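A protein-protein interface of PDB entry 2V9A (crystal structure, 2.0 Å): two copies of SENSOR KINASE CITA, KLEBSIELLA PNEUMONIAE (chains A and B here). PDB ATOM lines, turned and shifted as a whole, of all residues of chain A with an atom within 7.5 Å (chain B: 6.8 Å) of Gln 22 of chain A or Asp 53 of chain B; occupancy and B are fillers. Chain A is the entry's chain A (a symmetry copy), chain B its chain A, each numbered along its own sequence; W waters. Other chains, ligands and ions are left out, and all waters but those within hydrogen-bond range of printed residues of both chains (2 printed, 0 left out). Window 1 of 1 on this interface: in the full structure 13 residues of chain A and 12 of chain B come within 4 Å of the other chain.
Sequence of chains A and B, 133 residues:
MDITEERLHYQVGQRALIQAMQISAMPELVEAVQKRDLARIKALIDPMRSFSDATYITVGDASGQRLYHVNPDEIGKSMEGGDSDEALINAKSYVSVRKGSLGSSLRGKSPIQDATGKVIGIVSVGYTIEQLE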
ATOM      1  N   ARG A  15      14.273  -4.551 -20.771  1.00  0.00           N
ATOM      2  CA  ARG A  15      13.030  -4.246 -20.073  1.00  0.00           C
ATOM      3  C   ARG A  15      11.931  -5.207 -20.508  1.00  0.00           C
ATOM      4  O   ARG A  15      11.228  -5.780 -19.677  1.00  0.00           O
ATOM      5  CB  ARG A  15      12.596  -2.802 -20.332  1.00  0.00           C
ATOM      6  CG  ARG A  15      12.934  -1.835 -19.207  1.00  0.00           C
ATOM      7  CD  ARG A  15      12.310  -2.290 -17.896  1.00  0.00           C
ATOM      8  NE  ARG A  15      12.237  -1.214 -16.912  1.00  0.00           N
ATOM      9  CZ  ARG A  15      11.135  -0.520 -16.644  1.00  0.00           C
ATOM     10  NH1 ARG A  15      11.159   0.443 -15.732  1.00  0.00           N
ATOM     11  NH2 ARG A  15      10.007  -0.792 -17.284  1.00  0.00           N
ATOM     12  N   ALA A  16      11.792  -5.382 -21.818  1.00  0.00           N
ATOM     13  CA  ALA A  16      10.782  -6.275 -22.372  1.00  0.00           C
ATOM     14  C   ALA A  16      11.004  -7.713 -21.915  1.00  0.00           C
ATOM     15  O   ALA A  16      10.052  -8.419 -21.584  1.00  0.00           O
ATOM     16  CB  ALA A  16      10.780  -6.191 -23.892  1.00  0.00           C
ATOM     17  N   LEU A  17      12.263  -8.140 -21.902  1.00  0.00           N
ATOM     18  CA  LEU A  17      12.611  -9.500 -21.500  1.00  0.00           C
ATOM     19  C   LEU A  17      12.163  -9.798 -20.074  1.00  0.00           C
ATOM     20  O   LEU A  17      11.340 -10.685 -19.846  1.00  0.00           O
ATOM     21  CB  LEU A  17      14.117  -9.731 -21.630  1.00  0.00           C
ATOM     22  CG  LEU A  17      14.603 -11.125 -21.229  1.00  0.00           C
ATOM     23  CD1 LEU A  17      13.906 -12.190 -22.060  1.00  0.00           C
ATOM     24  CD2 LEU A  17      16.114 -11.234 -21.368  1.00  0.00           C
ATOM     25  N   ILE A  18      12.713  -9.057 -19.118  1.00  0.00           N
ATOM     26  CA  ILE A  18      12.366  -9.243 -17.713  1.00  0.00           C
ATOM     27  C   ILE A  18      10.856  -9.163 -17.519  1.00  0.00           C
ATOM     28  O   ILE A  18      10.245 -10.084 -16.981  1.00  0.00           O
ATOM     29  CB  ILE A  18      13.056  -8.197 -16.814  1.00  0.00           C
ATOM     30  CG1 ILE A  18      14.549  -8.116 -17.136  1.00  0.00           C
ATOM     31  CG2 ILE A  18      12.841  -8.531 -15.347  1.00  0.00           C
ATOM     32  CD1 ILE A  18      15.293  -7.072 -16.332  1.00  0.00           C
ATOM     33  N   GLN A  19      10.260  -8.062 -17.968  1.00  0.00           N
ATOM     34  CA  GLN A  19       8.816  -7.867 -17.864  1.00  0.00           C
ATOM     35  C   GLN A  19       8.048  -9.091 -18.353  1.00  0.00           C
ATOM     36  O   GLN A  19       7.077  -9.515 -17.727  1.00  0.00           O
ATOM     37  CB  GLN A  19       8.380  -6.628 -18.650  1.00  0.00           C
ATOM     38  CG  GLN A  19       8.711  -5.308 -17.972  1.00  0.00           C
ATOM     39  CD  GLN A  19       8.245  -4.107 -18.775  1.00  0.00           C
ATOM     40  OE1 GLN A  19       8.184  -2.989 -18.264  1.00  0.00           O
ATOM     41  NE2 GLN A  19       7.909  -4.337 -20.039  1.00  0.00           N
ATOM     42  N   ALA A  20       8.491  -9.655 -19.472  1.00  0.00           N
ATOM     43  CA  ALA A  20       7.857 -10.840 -20.036  1.00  0.00           C
ATOM     44  C   ALA A  20       7.949 -12.018 -19.074  1.00  0.00           C
ATOM     45  O   ALA A  20       6.949 -12.678 -18.788  1.00  0.00           O
ATOM     46  CB  ALA A  20       8.486 -11.195 -21.373  1.00  0.00           C
ATOM     47  N   MET A  21       9.155 -12.272 -18.576  1.00  0.00           N
ATOM     48  CA  MET A  21       9.389 -13.365 -17.641  1.00  0.00           C
ATOM     49  C   MET A  21       8.518 -13.240 -16.396  1.00  0.00           C
ATOM     50  O   MET A  21       8.019 -14.235 -15.875  1.00  0.00           O
ATOM     51  CB  MET A  21      10.863 -13.414 -17.230  1.00  0.00           C
ATOM     52  CG  MET A  21      11.823 -13.764 -18.354  1.00  0.00           C
ATOM     53  SD  MET A  21      13.519 -13.935 -17.765  1.00  0.00           S
ATOM     54  CE  MET A  21      14.370 -14.358 -19.282  1.00  0.00           C
ATOM     55  N   GLN A  22       8.341 -12.012 -15.921  1.00  0.00           N
ATOM     56  CA  GLN A  22       7.597 -11.768 -14.690  1.00  0.00           C
ATOM     57  C   GLN A  22       6.092 -11.911 -14.898  1.00  0.00           C
ATOM     58  O   GLN A  22       5.412 -12.593 -14.130  1.00  0.00           O
ATOM     59  CB  GLN A  22       7.920 -10.378 -14.141  1.00  0.00           C
ATOM     60  CG  GLN A  22       9.400 -10.028 -14.171  1.00  0.00           C
ATOM     61  CD  GLN A  22      10.248 -10.986 -13.358  1.00  0.00           C
ATOM     62  OE1 GLN A  22       9.821 -11.484 -12.317  1.00  0.00           O
ATOM     63  NE2 GLN A  22      11.464 -11.242 -13.827  1.00  0.00           N
ATOM     64  N   ILE A  23       5.576 -11.263 -15.937  1.00  0.00           N
ATOM     65  CA  ILE A  23       4.146 -11.285 -16.221  1.00  0.00           C
ATOM     66  C   ILE A  23       3.650 -12.696 -16.517  1.00  0.00           C
ATOM     67  O   ILE A  23       2.568 -13.086 -16.079  1.00  0.00           O
ATOM     68  CB  ILE A  23       3.792 -10.361 -17.402  1.00  0.00           C
ATOM     69  CG1 ILE A  23       4.140  -8.909 -17.065  1.00  0.00           C
ATOM     70  CG2 ILE A  23       2.321 -10.487 -17.753  1.00  0.00           C
ATOM     71  CD1 ILE A  23       3.879  -7.939 -18.196  1.00  0.00           C
ATOM     72  N   SER A  24       4.444 -13.462 -17.258  1.00  0.00           N
ATOM     73  CA  SER A  24       4.071 -14.826 -17.613  1.00  0.00           C
ATOM     74  C   SER A  24       4.299 -15.797 -16.458  1.00  0.00           C
ATOM     75  O   SER A  24       4.037 -16.992 -16.584  1.00  0.00           O
ATOM     76  CB  SER A  24       4.842 -15.292 -18.852  1.00  0.00           C
ATOM     77  OG  SER A  24       6.241 -15.227 -18.646  1.00  0.00           O
ATOM     78  N   ALA A  25       4.784 -15.279 -15.334  1.00  0.00           N
ATOM     79  CA  ALA A  25       5.085 -16.115 -14.175  1.00  0.00           C
ATOM     80  C   ALA A  25       4.061 -15.941 -13.059  1.00  0.00           C
ATOM     81  O   ALA A  25       4.000 -16.746 -12.131  1.00  0.00           O
ATOM     82  CB  ALA A  25       6.485 -15.818 -13.657  1.00  0.00           C
ATOM     83  N   MET A  26       3.257 -14.886 -13.154  1.00  0.00           N
ATOM     84  CA  MET A  26       2.268 -14.585 -12.125  1.00  0.00           C
ATOM     85  C   MET A  26       1.217 -15.683 -11.995  1.00  0.00           C
ATOM     86  O   MET A  26       0.596 -16.076 -12.982  1.00  0.00           O
ATOM     87  CB  MET A  26       1.599 -13.240 -12.402  1.00  0.00           C
ATOM     88  CG  MET A  26       2.531 -12.054 -12.238  1.00  0.00           C
ATOM     89  SD  MET A  26       1.743 -10.487 -12.641  1.00  0.00           S
ATOM     90  CE  MET A  26       3.023  -9.337 -12.145  1.00  0.00           C
ATOM     91  N   PRO A  27       1.019 -16.177 -10.764  1.00  0.00           N
ATOM     92  CA  PRO A  27       0.073 -17.253 -10.447  1.00  0.00           C
ATOM     93  C   PRO A  27      -1.358 -16.876 -10.813  1.00  0.00           C
ATOM     94  O   PRO A  27      -2.112 -17.720 -11.296  1.00  0.00           O
ATOM     95  CB  PRO A  27       0.203 -17.397  -8.927  1.00  0.00           C
ATOM     96  CG  PRO A  27       1.533 -16.815  -8.596  1.00  0.00           C
ATOM     97  CD  PRO A  27       1.727 -15.698  -9.566  1.00  0.00           C
ATOM     98  N   LEU A  29      -2.302 -15.027 -13.205  1.00  0.00           N
ATOM     99  CA  LEU A  29      -2.416 -15.165 -14.649  1.00  0.00           C
ATOM    100  C   LEU A  29      -2.334 -16.636 -15.043  1.00  0.00           C
ATOM    101  O   LEU A  29      -3.065 -17.093 -15.920  1.00  0.00           O
ATOM    102  CB  LEU A  29      -1.324 -14.361 -15.356  1.00  0.00           C
ATOM    103  CG  LEU A  29      -1.595 -13.997 -16.817  1.00  0.00           C
ATOM    104  CD1 LEU A  29      -2.895 -13.220 -16.940  1.00  0.00           C
ATOM    105  CD2 LEU A  29      -0.437 -13.202 -17.398  1.00  0.00           C
ATOM    106  N   MET A  48      -1.170  -2.955 -16.145  1.00  0.00           N
ATOM    107  CA  MET A  48       0.225  -3.055 -16.569  1.00  0.00           C
ATOM    108  C   MET A  48       0.534  -2.200 -17.796  1.00  0.00           C
ATOM    109  O   MET A  48       1.653  -1.711 -17.954  1.00  0.00           O
ATOM    110  CB  MET A  48       0.596  -4.513 -16.849  1.00  0.00           C
ATOM    111  CG  MET A  48       0.464  -5.427 -15.645  1.00  0.00           C
ATOM    112  SD  MET A  48       0.958  -7.121 -16.008  1.00  0.00           S
ATOM    113  CE  MET A  48       0.650  -7.902 -14.428  1.00  0.00           C
ATOM    114  N   SER A 110       8.061 -14.553 -23.192  1.00  0.00           N
ATOM    115  CA  SER A 110       8.284 -15.635 -22.240  1.00  0.00           C
ATOM    116  C   SER A 110       7.046 -16.520 -22.137  1.00  0.00           C
ATOM    117  O   SER A 110       5.920 -16.021 -22.124  1.00  0.00           O
ATOM    118  CB  SER A 110       8.652 -15.078 -20.863  1.00  0.00           C
ATOM    119  OG  SER A 110       8.894 -16.123 -19.939  1.00  0.00           O
ATOM    120  N   VAL A 123       3.493 -14.997 -23.171  1.00  0.00           N
ATOM    121  CA  VAL A 123       3.387 -13.556 -22.973  1.00  0.00           C
ATOM    122  C   VAL A 123       4.326 -12.814 -23.917  1.00  0.00           C
ATOM    123  O   VAL A 123       5.480 -13.204 -24.091  1.00  0.00           O
ATOM    124  CB  VAL A 123       3.696 -13.158 -21.517  1.00  0.00           C
ATOM    125  CG1 VAL A 123       4.062 -11.684 -21.431  1.00  0.00           C
ATOM    126  CG2 VAL A 123       2.511 -13.477 -20.616  1.00  0.00           C
ATOM    127  N   VAL B  12      17.784  -8.140 -11.201  1.00  0.00           N
ATOM    128  CA  VAL B  12      16.534  -8.454 -10.524  1.00  0.00           C
ATOM    129  C   VAL B  12      16.729  -8.505  -9.013  1.00  0.00           C
ATOM    130  O   VAL B  12      15.938  -7.944  -8.255  1.00  0.00           O
ATOM    131  CB  VAL B  12      15.976  -9.807 -10.998  1.00  0.00           C
ATOM    132  CG1 VAL B  12      15.033 -10.383  -9.963  1.00  0.00           C
ATOM    133  CG2 VAL B  12      15.286  -9.657 -12.346  1.00  0.00           C
ATOM    134  N   ARG B  15      16.628  -5.240  -7.342  1.00  0.00           N
ATOM    135  CA  ARG B  15      15.264  -4.729  -7.369  1.00  0.00           C
ATOM    136  C   ARG B  15      14.456  -5.319  -6.220  1.00  0.00           C
ATOM    137  O   ARG B  15      13.775  -4.598  -5.493  1.00  0.00           O
ATOM    138  CB  ARG B  15      14.586  -5.046  -8.703  1.00  0.00           C
ATOM    139  CG  ARG B  15      14.557  -3.883  -9.684  1.00  0.00           C
ATOM    140  CD  ARG B  15      13.859  -2.677  -9.072  1.00  0.00           C
ATOM    141  NE  ARG B  15      13.431  -1.713 -10.082  1.00  0.00           N
ATOM    142  CZ  ARG B  15      12.184  -1.606 -10.531  1.00  0.00           C
ATOM    143  NH1 ARG B  15      11.881  -0.699 -11.450  1.00  0.00           N
ATOM    144  NH2 ARG B  15      11.237  -2.403 -10.057  1.00  0.00           N
ATOM    145  N   GLN B  19      13.060  -3.050  -3.012  1.00  0.00           N
ATOM    146  CA  GLN B  19      11.607  -3.156  -2.908  1.00  0.00           C
ATOM    147  C   GLN B  19      11.182  -3.751  -1.570  1.00  0.00           C
ATOM    148  O   GLN B  19      10.239  -3.273  -0.940  1.00  0.00           O
ATOM    149  CB  GLN B  19      11.043  -3.995  -4.057  1.00  0.00           C
ATOM    150  CG  GLN B  19      10.999  -3.275  -5.396  1.00  0.00           C
ATOM    151  CD  GLN B  19      10.416  -4.136  -6.501  1.00  0.00           C
ATOM    152  OE1 GLN B  19      10.058  -3.639  -7.569  1.00  0.00           O
ATOM    153  NE2 GLN B  19      10.317  -5.436  -6.248  1.00  0.00           N
ATOM    154  N   MET B  48       0.689  -2.894  -5.652  1.00  0.00           N
ATOM    155  CA  MET B  48       2.121  -3.112  -5.849  1.00  0.00           C
ATOM    156  C   MET B  48       2.419  -4.280  -6.785  1.00  0.00           C
ATOM    157  O   MET B  48       3.426  -4.274  -7.494  1.00  0.00           O
ATOM    158  CB  MET B  48       2.816  -3.337  -4.505  1.00  0.00           C
ATOM    159  CG  MET B  48       2.705  -2.166  -3.546  1.00  0.00           C
ATOM    160  SD  MET B  48       3.581  -2.455  -1.998  1.00  0.00           S
ATOM    161  CE  MET B  48       3.218  -0.936  -1.124  1.00  0.00           C
ATOM    162  N   ARG B  49       1.546  -5.282  -6.781  1.00  0.00           N
ATOM    163  CA  ARG B  49       1.732  -6.460  -7.621  1.00  0.00           C
ATOM    164  C   ARG B  49       1.824  -6.080  -9.096  1.00  0.00           C
ATOM    165  O   ARG B  49       2.825  -6.359  -9.757  1.00  0.00           O
ATOM    166  CB  ARG B  49       0.595  -7.460  -7.404  1.00  0.00           C
ATOM    167  N   SER B  50       0.775  -5.443  -9.606  1.00  0.00           N
ATOM    168  CA  SER B  50       0.741  -5.014 -10.998  1.00  0.00           C
ATOM    169  C   SER B  50       1.770  -3.915 -11.249  1.00  0.00           C
ATOM    170  O   SER B  50       2.351  -3.828 -12.331  1.00  0.00           O
ATOM    171  CB  SER B  50      -0.659  -4.523 -11.370  1.00  0.00           C
ATOM    172  OG  SER B  50      -1.635  -5.517 -11.111  1.00  0.00           O
ATOM    173  N   PHE B  51       1.984  -3.080 -10.238  1.00  0.00           N
ATOM    174  CA  PHE B  51       2.950  -1.989 -10.317  1.00  0.00           C
ATOM    175  C   PHE B  51       4.335  -2.507 -10.685  1.00  0.00           C
ATOM    176  O   PHE B  51       4.856  -2.213 -11.760  1.00  0.00           O
ATOM    177  CB  PHE B  51       3.021  -1.257  -8.974  1.00  0.00           C
ATOM    178  CG  PHE B  51       1.789  -0.464  -8.648  1.00  0.00           C
ATOM    179  CD1 PHE B  51       0.663  -0.541  -9.448  1.00  0.00           C
ATOM    180  CD2 PHE B  51       1.747   0.340  -7.522  1.00  0.00           C
ATOM    181  CE1 PHE B  51      -0.473   0.181  -9.145  1.00  0.00           C
ATOM    182  CE2 PHE B  51       0.612   1.062  -7.212  1.00  0.00           C
ATOM    183  CZ  PHE B  51      -0.499   0.983  -8.026  1.00  0.00           C
ATOM    184  N   SER B  52       4.923  -3.281  -9.778  1.00  0.00           N
ATOM    185  CA  SER B  52       6.268  -3.809  -9.965  1.00  0.00           C
ATOM    186  C   SER B  52       6.270  -5.048 -10.851  1.00  0.00           C
ATOM    187  O   SER B  52       5.251  -5.724 -10.997  1.00  0.00           O
ATOM    188  CB  SER B  52       6.896  -4.142  -8.610  1.00  0.00           C
ATOM    189  OG  SER B  52       6.146  -5.135  -7.934  1.00  0.00           O
ATOM    190  N   ASP B  53       7.424  -5.341 -11.441  1.00  0.00           N
ATOM    191  CA  ASP B  53       7.591  -6.535 -12.259  1.00  0.00           C
ATOM    192  C   ASP B  53       7.947  -7.715 -11.363  1.00  0.00           C
ATOM    193  O   ASP B  53       8.759  -8.566 -11.726  1.00  0.00           O
ATOM    194  N   ALA B  54       7.333  -7.752 -10.186  1.00  0.00           N
ATOM    195  CA  ALA B  54       7.581  -8.813  -9.222  1.00  0.00           C
ATOM    196  C   ALA B  54       6.600  -9.959  -9.426  1.00  0.00           C
ATOM    197  O   ALA B  54       5.387  -9.751  -9.453  1.00  0.00           O
ATOM    198  CB  ALA B  54       7.478  -8.274  -7.805  1.00  0.00           C
ATOM    199  N   THR B  55       7.132 -11.167  -9.576  1.00  0.00           N
ATOM    200  CA  THR B  55       6.301 -12.348  -9.757  1.00  0.00           C
ATOM    201  C   THR B  55       5.278 -12.451  -8.633  1.00  0.00           C
ATOM    202  O   THR B  55       4.095 -12.689  -8.877  1.00  0.00           O
ATOM    203  CB  THR B  55       7.149 -13.631  -9.802  1.00  0.00           C
ATOM    204  OG1 THR B  55       8.171 -13.496 -10.798  1.00  0.00           O
ATOM    205  CG2 THR B  55       6.280 -14.832 -10.137  1.00  0.00           C
ATOM    206  N   TYR B  56       5.739 -12.266  -7.400  1.00  0.00           N
ATOM    207  CA  TYR B  56       4.848 -12.276  -6.246  1.00  0.00           C
ATOM    208  C   TYR B  56       5.362 -11.387  -5.122  1.00  0.00           C
ATOM    209  O   TYR B  56       6.519 -10.969  -5.121  1.00  0.00           O
ATOM    210  CB  TYR B  56       4.639 -13.703  -5.732  1.00  0.00           C
ATOM    211  CG  TYR B  56       5.864 -14.327  -5.101  1.00  0.00           C
ATOM    212  CD1 TYR B  56       6.097 -14.220  -3.735  1.00  0.00           C
ATOM    213  CD2 TYR B  56       6.784 -15.030  -5.868  1.00  0.00           C
ATOM    214  CE1 TYR B  56       7.213 -14.790  -3.153  1.00  0.00           C
ATOM    215  CE2 TYR B  56       7.903 -15.603  -5.293  1.00  0.00           C
ATOM    216  CZ  TYR B  56       8.112 -15.480  -3.936  1.00  0.00           C
ATOM    217  OH  TYR B  56       9.223 -16.050  -3.359  1.00  0.00           O
ATOM    218  N   GLY B 126       9.029 -11.591  -4.529  1.00  0.00           N
ATOM    219  CA  GLY B 126       9.582 -12.632  -5.377  1.00  0.00           C
ATOM    220  C   GLY B 126       9.743 -12.249  -6.836  1.00  0.00           C
ATOM    221  O   GLY B 126       8.971 -11.456  -7.376  1.00  0.00           O
ATOM    222  N   TYR B 127      10.758 -12.825  -7.472  1.00  0.00           N
ATOM    223  CA  TYR B 127      11.033 -12.598  -8.887  1.00  0.00           C
ATOM    224  C   TYR B 127      11.411 -13.912  -9.563  1.00  0.00           C
ATOM    225  O   TYR B 127      11.715 -14.896  -8.891  1.00  0.00           O
ATOM    226  CB  TYR B 127      12.164 -11.585  -9.056  1.00  0.00           C
ATOM    227  CG  TYR B 127      11.722 -10.139  -9.013  1.00  0.00           C
ATOM    228  CD1 TYR B 127      11.636  -9.386 -10.177  1.00  0.00           C
ATOM    229  CD2 TYR B 127      11.395  -9.525  -7.813  1.00  0.00           C
ATOM    230  CE1 TYR B 127      11.237  -8.065 -10.147  1.00  0.00           C
ATOM    231  CE2 TYR B 127      10.994  -8.202  -7.773  1.00  0.00           C
ATOM    232  CZ  TYR B 127      10.916  -7.479  -8.943  1.00  0.00           C
ATOM    233  OH  TYR B 127      10.517  -6.163  -8.910  1.00  0.00           O
ATOM    234  N   THR B 128      11.396 -13.924 -10.893  1.00  0.00           N
ATOM    235  CA  THR B 128      11.704 -15.138 -11.644  1.00  0.00           C
ATOM    236  C   THR B 128      12.582 -14.856 -12.862  1.00  0.00           C
ATOM    237  O   THR B 128      12.400 -13.853 -13.551  1.00  0.00           O
ATOM    238  CB  THR B 128      10.420 -15.858 -12.105  1.00  0.00           C
ATOM    239  OG1 THR B 128       9.549 -16.056 -10.985  1.00  0.00           O
ATOM    240  CG2 THR B 128      10.754 -17.206 -12.727  1.00  0.00           C
ATOM    241  N   ILE B 129      13.534 -15.749 -13.118  1.00  0.00           N
ATOM    242  CA  ILE B 129      14.419 -15.624 -14.270  1.00  0.00           C
ATOM    243  C   ILE B 129      14.363 -16.875 -15.141  1.00  0.00           C
ATOM    244  O   ILE B 129      15.003 -17.883 -14.835  1.00  0.00           O
ATOM    245  CB  ILE B 129      15.880 -15.379 -13.840  1.00  0.00           C
ATOM    246  CG1 ILE B 129      16.003 -14.050 -13.092  1.00  0.00           C
ATOM    247  CG2 ILE B 129      16.802 -15.388 -15.049  1.00  0.00           C
ATOM    248  CD1 ILE B 129      15.634 -12.847 -13.929  1.00  0.00           C
ATOM    249  N   GLU B 130      13.597 -16.808 -16.225  1.00  0.00           N
ATOM    250  CA  GLU B 130      13.488 -17.929 -17.151  1.00  0.00           C
ATOM    251  C   GLU B 130      14.676 -17.971 -18.108  1.00  0.00           C
ATOM    252  O   GLU B 130      15.342 -18.998 -18.242  1.00  0.00           O
ATOM    253  CB  GLU B 130      12.179 -17.859 -17.940  1.00  0.00           C
ATOM    254  CG  GLU B 130      10.927 -18.025 -17.095  1.00  0.00           C
ATOM    255  CD  GLU B 130       9.707 -18.370 -17.927  1.00  0.00           C
ATOM    256  OE1 GLU B 130       9.877 -18.853 -19.065  1.00  0.00           O
ATOM    257  OE2 GLU B 130       8.576 -18.165 -17.442  1.00  0.00           O
HETATM  258  O   HOH W   1       9.159  -0.273 -13.394  1.00  0.00           O
HETATM  259  O   HOH W   2       7.024 -16.522 -16.544  1.00  0.00           O
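Positions printed for both chains: 15, 19 and 48.
Of the 13 pairs that touch across the chains among the printed residues, none has its exchanged pair printed and touching as well.
Ile 129 of chain B touches Met 21 of chain A.
Gln 22 of chain A touches Tyr 127 of chain B (OE1 to CD1, 3.5 Å).
OG of Ser 24 of chain A touches OE2 of Glu 130 of chain B, 3.9 Å away.
Ala 25 of chain A touches Thr 55 of chain B.
Arg 49 of chain B touches Met 26 of chain A.
CE of Met 26 of chain A touches O of Ala 54 of chain B, at 3.6 Å.
Met 26 of chain A touches Thr 55 of chain B.
Pro 27 of chain A touches Thr 55 of chain B.
Gln 19 of chain A touches none of the printed residues of chain B.
Of the printed residues of chain B, Ala 25 of chain A touches Thr 55.
Asp 53 of chain B touches just one residue of chain A: Gln 22 (2.9 Å).
Of the printed residues of chain A, Ala 54 of chain B touches Met 26 (3.6 Å).
Of the printed residues of chain A, Thr 55 of chain B touches Gln 22 (3.0 Å), Ala 25 (3.6 Å), Met 26 (3.8 Å) and Pro 27 (3.9 Å).
Of the printed residues of chain A, Ile 129 of chain B touches Met 21 (3.98 Å).
The nearest residue of chain A that does not touch Asp 53 of chain B is Met 26 of chain A (5.2 Å).
The nearest printed residue of chain A that does not touch Thr 128 of chain B is Met 21 of chain A (4.01 Å).
Water W2 lies within hydrogen-bond range of the side-chain carboxylate (OE2) of Glu 130 of chain B, the backbone carbonyl oxygen (O) of Met 21 of chain A, the side-chain hydroxyl (OG) of Ser 24 of chain A and the backbone NH (N) of Ala 25 of chain A.
Water W1 lies within hydrogen-bond range of the guanidinium group (NH1) of Arg 15 of chain A and the guanidinium group (NH1) of Arg 15 of chain B.
The side-chain hydroxyl (OH) of Tyr 127 of chain B sits at hydrogen-bond distance from the side-chain amide nitrogen (NE2) of Gln 19 of chain B (2.8 Å).
The backbone carbonyl oxygen of Gly 126 of chain B lies within hydrogen-bond range of the backbone NH of Thr 55 of chain B (2.9 Å).
OG1 of Thr 55 of chain B sits at hydrogen-bond distance from OG1 of Thr 128 of chain B (2.9 Å).
The side-chain hydroxyl (OG) of Ser 24 of chain A lies within hydrogen-bond range of the backbone carbonyl oxygen (O) of Ala 20 of chain A, at 2.6 Å.
The side-chain hydroxyl (OG) of Ser 24 of chain A lies within hydrogen-bond range of the side-chain hydroxyl (OG) of Ser 110 of chain A (3.1 Å).
The backbone NH of Val 123 of chain A lies within hydrogen-bond range of the backbone carbonyl oxygen of Ser 110 of chain A (2.8 Å).
The backbone carbonyl oxygen of Asp 53 of chain B sits close to the side-chain amide oxygen of Gln 22 of chain A, 3.2 Å away.
The side-chain hydroxyl (OG1) of Thr 55 of chain B lies within hydrogen-bond range of the side-chain amide oxygen (OE1) of Gln 22 of chain A, at 3.0 Å.
The side-chain amide nitrogen (NE2) of Gln 22 of chain A sits at hydrogen-bond distance from the backbone carbonyl oxygen (O) of Thr 128 of chain B (2.8 Å).
The side-chain sulfur of Met 21 of chain A lies within hydrogen-bond range of the backbone NH of Glu 130 of chain B, 3.3 Å away.
The side-chain carboxylate (OE1) of Glu 130 of chain B lies within hydrogen-bond range of the side-chain hydroxyl (OG) of Ser 110 of chain A (3.0 Å).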
